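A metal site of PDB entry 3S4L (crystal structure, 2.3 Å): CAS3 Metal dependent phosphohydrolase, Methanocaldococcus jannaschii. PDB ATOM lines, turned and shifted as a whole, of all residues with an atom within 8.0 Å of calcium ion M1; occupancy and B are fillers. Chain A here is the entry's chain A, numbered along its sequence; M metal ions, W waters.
A ring nitrogen (ND1) of His 123 lies within hydrogen-bond range of the backbone carbonyl oxygen of Val 120 (2.5 Å). OG of Ser 95 lies within hydrogen-bond range of O of His 91 (3.3 Å). A ring nitrogen (ND1) of His 91 sits at hydrogen-bond distance from the side-chain carboxylate of Glu 92, 3.3 Å away. OD1 of Asp 67 lies within salt-bridge range of NZ of Lys 70, at 3.9 Å.
The nearest printed residue that does not touch calcium ion M1 is Lys 70 (4.5 Å).
Calcium ion M1 is bound by the side-chain carboxylate of Asp 67 (2.3 Å), a ring nitrogen (NE2) of His 91 (2.3 Å), water W1 (2.3 Å), a ring nitrogen (NE2) of His 124 (2.3 Å), a ring nitrogen (NE2) of His 123 (2.4 Å) and water W2 (2.8 Å).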
ATOM      1  N   PHE A  12      -7.249  -9.289  16.853  1.00  0.00           N
ATOM      2  CA  PHE A  12      -5.833  -9.150  17.194  1.00  0.00           C
ATOM      3  C   PHE A  12      -5.183 -10.516  17.015  1.00  0.00           C
ATOM      4  O   PHE A  12      -5.875 -11.538  16.990  1.00  0.00           O
ATOM      5  CB  PHE A  12      -5.651  -8.742  18.657  1.00  0.00           C
ATOM      6  CG  PHE A  12      -6.472  -7.562  19.067  1.00  0.00           C
ATOM      7  CD1 PHE A  12      -5.999  -6.275  18.854  1.00  0.00           C
ATOM      8  CD2 PHE A  12      -7.707  -7.731  19.666  1.00  0.00           C
ATOM      9  CE1 PHE A  12      -6.764  -5.179  19.239  1.00  0.00           C
ATOM     10  CE2 PHE A  12      -8.472  -6.643  20.046  1.00  0.00           C
ATOM     11  CZ  PHE A  12      -7.998  -5.356  19.833  1.00  0.00           C
ATOM     12  N   HIS A  20     -13.985 -11.044  20.513  1.00  0.00           N
ATOM     13  CA  HIS A  20     -13.738  -9.671  20.929  1.00  0.00           C
ATOM     14  C   HIS A  20     -15.044  -8.854  20.970  1.00  0.00           C
ATOM     15  O   HIS A  20     -15.254  -8.058  21.890  1.00  0.00           O
ATOM     16  CB  HIS A  20     -12.726  -9.017  19.977  1.00  0.00           C
ATOM     17  CG  HIS A  20     -12.468  -7.580  20.275  1.00  0.00           C
ATOM     18  ND1 HIS A  20     -12.214  -7.112  21.553  1.00  0.00           N
ATOM     19  CD2 HIS A  20     -12.398  -6.493  19.468  1.00  0.00           C
ATOM     20  CE1 HIS A  20     -12.027  -5.811  21.517  1.00  0.00           C
ATOM     21  NE2 HIS A  20     -12.123  -5.410  20.261  1.00  0.00           N
ATOM     22  N   MET A  24     -17.114  -7.092  24.275  1.00  0.00           N
ATOM     23  CA  MET A  24     -17.494  -5.688  24.325  1.00  0.00           C
ATOM     24  C   MET A  24     -18.998  -5.533  24.591  1.00  0.00           C
ATOM     25  O   MET A  24     -19.441  -4.599  25.253  1.00  0.00           O
ATOM     26  CB  MET A  24     -17.093  -4.996  23.021  1.00  0.00           C
ATOM     27  CG  MET A  24     -15.633  -4.561  22.945  1.00  0.00           C
ATOM     28  SD  MET A  24     -15.263  -3.780  21.360  1.00  0.00           S
ATOM     29  CE  MET A  24     -14.206  -2.424  21.871  1.00  0.00           C
ATOM     30  N   LEU A  65     -20.233  -3.543  14.981  1.00  0.00           N
ATOM     31  CA  LEU A  65     -19.799  -3.306  13.618  1.00  0.00           C
ATOM     32  C   LEU A  65     -18.628  -2.335  13.485  1.00  0.00           C
ATOM     33  O   LEU A  65     -18.076  -2.187  12.395  1.00  0.00           O
ATOM     34  CB  LEU A  65     -20.975  -2.836  12.777  1.00  0.00           C
ATOM     35  CG  LEU A  65     -22.120  -3.838  12.568  1.00  0.00           C
ATOM     36  CD1 LEU A  65     -23.194  -3.193  11.674  1.00  0.00           C
ATOM     37  CD2 LEU A  65     -21.602  -5.141  11.927  1.00  0.00           C
ATOM     38  N   HIS A  66     -18.262  -1.647  14.566  1.00  0.00           N
ATOM     39  CA  HIS A  66     -17.273  -0.592  14.370  1.00  0.00           C
ATOM     40  C   HIS A  66     -15.913  -1.125  13.871  1.00  0.00           C
ATOM     41  O   HIS A  66     -15.167  -0.398  13.225  1.00  0.00           O
ATOM     42  CB  HIS A  66     -17.146   0.320  15.583  1.00  0.00           C
ATOM     43  CG  HIS A  66     -16.458  -0.305  16.750  1.00  0.00           C
ATOM     44  ND1 HIS A  66     -17.093  -1.202  17.588  1.00  0.00           N
ATOM     45  CD2 HIS A  66     -15.197  -0.177  17.233  1.00  0.00           C
ATOM     46  CE1 HIS A  66     -16.250  -1.590  18.531  1.00  0.00           C
ATOM     47  NE2 HIS A  66     -15.094  -0.982  18.331  1.00  0.00           N
ATOM     48  N   ASP A  67     -15.617  -2.388  14.160  1.00  0.00           N
ATOM     49  CA  ASP A  67     -14.404  -3.014  13.638  1.00  0.00           C
ATOM     50  C   ASP A  67     -14.638  -4.065  12.581  1.00  0.00           C
ATOM     51  O   ASP A  67     -13.751  -4.891  12.308  1.00  0.00           O
ATOM     52  CB  ASP A  67     -13.584  -3.626  14.783  1.00  0.00           C
ATOM     53  CG  ASP A  67     -12.767  -2.591  15.531  1.00  0.00           C
ATOM     54  OD1 ASP A  67     -12.384  -2.863  16.684  1.00  0.00           O
ATOM     55  OD2 ASP A  67     -12.526  -1.518  14.931  1.00  0.00           O
ATOM     56  N   ILE A  68     -15.828  -4.056  11.983  1.00  0.00           N
ATOM     57  CA  ILE A  68     -16.132  -5.038  10.932  1.00  0.00           C
ATOM     58  C   ILE A  68     -15.150  -4.878   9.770  1.00  0.00           C
ATOM     59  O   ILE A  68     -14.829  -5.845   9.084  1.00  0.00           O
ATOM     60  CB  ILE A  68     -17.609  -4.979  10.464  1.00  0.00           C
ATOM     61  CG1 ILE A  68     -17.979  -6.267   9.741  1.00  0.00           C
ATOM     62  CG2 ILE A  68     -17.831  -3.763   9.599  1.00  0.00           C
ATOM     63  CD1 ILE A  68     -17.477  -7.520  10.452  1.00  0.00           C
ATOM     64  N   GLY A  69     -14.646  -3.648   9.585  1.00  0.00           N
ATOM     65  CA  GLY A  69     -13.648  -3.358   8.566  1.00  0.00           C
ATOM     66  C   GLY A  69     -12.396  -4.219   8.705  1.00  0.00           C
ATOM     67  O   GLY A  69     -11.625  -4.395   7.750  1.00  0.00           O
ATOM     68  N   LYS A  70     -12.184  -4.774   9.909  1.00  0.00           N
ATOM     69  CA  LYS A  70     -11.071  -5.692  10.107  1.00  0.00           C
ATOM     70  C   LYS A  70     -11.235  -6.998   9.326  1.00  0.00           C
ATOM     71  O   LYS A  70     -10.256  -7.713   9.076  1.00  0.00           O
ATOM     72  CB  LYS A  70     -10.851  -5.988  11.594  1.00  0.00           C
ATOM     73  CG  LYS A  70     -10.252  -4.825  12.403  1.00  0.00           C
ATOM     74  CD  LYS A  70     -10.069  -5.221  13.900  1.00  0.00           C
ATOM     75  CE  LYS A  70      -9.488  -4.082  14.750  1.00  0.00           C
ATOM     76  NZ  LYS A  70      -8.989  -4.597  16.082  1.00  0.00           N
ATOM     77  N   TYR A  75      -6.557  -6.337   6.056  1.00  0.00           N
ATOM     78  CA  TYR A  75      -6.389  -6.217   7.500  1.00  0.00           C
ATOM     79  C   TYR A  75      -6.021  -7.582   8.119  1.00  0.00           C
ATOM     80  O   TYR A  75      -5.114  -7.686   8.950  1.00  0.00           O
ATOM     81  CB  TYR A  75      -7.624  -5.589   8.185  1.00  0.00           C
ATOM     82  CG  TYR A  75      -7.252  -5.043   9.552  1.00  0.00           C
ATOM     83  CD1 TYR A  75      -7.130  -5.897  10.661  1.00  0.00           C
ATOM     84  CD2 TYR A  75      -6.954  -3.705   9.724  1.00  0.00           C
ATOM     85  CE1 TYR A  75      -6.739  -5.402  11.915  1.00  0.00           C
ATOM     86  CE2 TYR A  75      -6.554  -3.193  10.967  1.00  0.00           C
ATOM     87  CZ  TYR A  75      -6.448  -4.052  12.062  1.00  0.00           C
ATOM     88  OH  TYR A  75      -6.068  -3.558  13.294  1.00  0.00           O
ATOM     89  N   ARG A  90      -7.342   1.956   6.154  1.00  0.00           N
ATOM     90  CA  ARG A  90      -8.072   2.324   7.376  1.00  0.00           C
ATOM     91  C   ARG A  90      -9.397   1.564   7.488  1.00  0.00           C
ATOM     92  O   ARG A  90     -10.361   1.848   6.780  1.00  0.00           O
ATOM     93  CB  ARG A  90      -8.299   3.836   7.422  1.00  0.00           C
ATOM     94  CG  ARG A  90      -7.021   4.618   7.196  1.00  0.00           C
ATOM     95  CD  ARG A  90      -6.338   5.032   8.484  1.00  0.00           C
ATOM     96  NE  ARG A  90      -6.417   4.045   9.548  1.00  0.00           N
ATOM     97  CZ  ARG A  90      -6.725   4.335  10.801  1.00  0.00           C
ATOM     98  NH1 ARG A  90      -7.010   5.584  11.138  1.00  0.00           N
ATOM     99  NH2 ARG A  90      -6.768   3.369  11.728  1.00  0.00           N
ATOM    100  N   HIS A  91      -9.411   0.566   8.373  1.00  0.00           N
ATOM    101  CA  HIS A  91     -10.558  -0.328   8.514  1.00  0.00           C
ATOM    102  C   HIS A  91     -11.862   0.402   8.804  1.00  0.00           C
ATOM    103  O   HIS A  91     -12.940  -0.026   8.363  1.00  0.00           O
ATOM    104  CB  HIS A  91     -10.291  -1.328   9.624  1.00  0.00           C
ATOM    105  CG  HIS A  91     -10.155  -0.708  10.979  1.00  0.00           C
ATOM    106  ND1 HIS A  91      -9.021  -0.060  11.403  1.00  0.00           N
ATOM    107  CD2 HIS A  91     -11.038  -0.640  12.009  1.00  0.00           C
ATOM    108  CE1 HIS A  91      -9.202   0.389  12.636  1.00  0.00           C
ATOM    109  NE2 HIS A  91     -10.407   0.054  13.020  1.00  0.00           N
ATOM    110  N   GLU A  92     -11.788   1.522   9.532  1.00  0.00           N
ATOM    111  CA  GLU A  92     -13.016   2.189   9.974  1.00  0.00           C
ATOM    112  C   GLU A  92     -13.861   2.741   8.830  1.00  0.00           C
ATOM    113  O   GLU A  92     -15.085   2.895   8.977  1.00  0.00           O
ATOM    114  CB  GLU A  92     -12.729   3.288  11.016  1.00  0.00           C
ATOM    115  CG  GLU A  92     -11.829   4.410  10.553  1.00  0.00           C
ATOM    116  CD  GLU A  92     -10.370   4.183  10.948  1.00  0.00           C
ATOM    117  OE1 GLU A  92      -9.851   3.069  10.721  1.00  0.00           O
ATOM    118  OE2 GLU A  92      -9.750   5.113  11.494  1.00  0.00           O
ATOM    119  N   SER A  95     -15.797  -0.154   7.822  1.00  0.00           N
ATOM    120  CA  SER A  95     -16.812  -0.327   8.873  1.00  0.00           C
ATOM    121  C   SER A  95     -17.997   0.642   8.696  1.00  0.00           C
ATOM    122  O   SER A  95     -19.173   0.241   8.760  1.00  0.00           O
ATOM    123  CB  SER A  95     -16.220  -0.123  10.282  1.00  0.00           C
ATOM    124  OG  SER A  95     -15.193  -1.058  10.602  1.00  0.00           O
ATOM    125  N   VAL A 120     -18.728   5.566  13.635  1.00  0.00           N
ATOM    126  CA  VAL A 120     -17.887   4.434  13.310  1.00  0.00           C
ATOM    127  C   VAL A 120     -16.672   4.844  12.447  1.00  0.00           C
ATOM    128  O   VAL A 120     -15.568   4.325  12.621  1.00  0.00           O
ATOM    129  CB  VAL A 120     -18.705   3.351  12.587  1.00  0.00           C
ATOM    130  CG1 VAL A 120     -17.771   2.435  11.790  1.00  0.00           C
ATOM    131  CG2 VAL A 120     -19.538   2.545  13.600  1.00  0.00           C
ATOM    132  N   HIS A 123     -14.251   6.391  14.874  1.00  0.00           N
ATOM    133  CA  HIS A 123     -14.079   5.765  16.183  1.00  0.00           C
ATOM    134  C   HIS A 123     -12.621   5.697  16.620  1.00  0.00           C
ATOM    135  O   HIS A 123     -12.335   5.244  17.732  1.00  0.00           O
ATOM    136  CB  HIS A 123     -14.778   4.398  16.312  1.00  0.00           C
ATOM    137  CG  HIS A 123     -14.078   3.284  15.585  1.00  0.00           C
ATOM    138  ND1 HIS A 123     -14.463   2.871  14.330  1.00  0.00           N
ATOM    139  CD2 HIS A 123     -13.053   2.490  15.960  1.00  0.00           C
ATOM    140  CE1 HIS A 123     -13.706   1.861  13.951  1.00  0.00           C
ATOM    141  NE2 HIS A 123     -12.827   1.611  14.921  1.00  0.00           N
ATOM    142  N   HIS A 124     -11.702   6.138  15.772  1.00  0.00           N
ATOM    143  CA  HIS A 124     -10.322   6.191  16.226  1.00  0.00           C
ATOM    144  C   HIS A 124      -9.808   7.537  16.718  1.00  0.00           C
ATOM    145  O   HIS A 124      -8.939   7.561  17.601  1.00  0.00           O
ATOM    146  CB  HIS A 124      -9.356   5.470  15.283  1.00  0.00           C
ATOM    147  CG  HIS A 124      -9.270   4.019  15.584  1.00  0.00           C
ATOM    148  ND1 HIS A 124      -8.548   3.527  16.638  1.00  0.00           N
ATOM    149  CD2 HIS A 124      -9.930   2.968  15.045  1.00  0.00           C
ATOM    150  CE1 HIS A 124      -8.713   2.218  16.713  1.00  0.00           C
ATOM    151  NE2 HIS A 124      -9.538   1.855  15.752  1.00  0.00           N
HETATM  152 CA    CA M   1     -11.012   0.127  15.242  1.00  0.00          CA
HETATM  153 CA    CA M   2     -12.467   0.916  20.692  1.00  0.00          CA
HETATM  154  O   HOH W   1     -11.655  -0.469  17.387  1.00  0.00           O
HETATM  155  O   HOH W   2      -9.104  -1.608  16.389  1.00  0.00           O
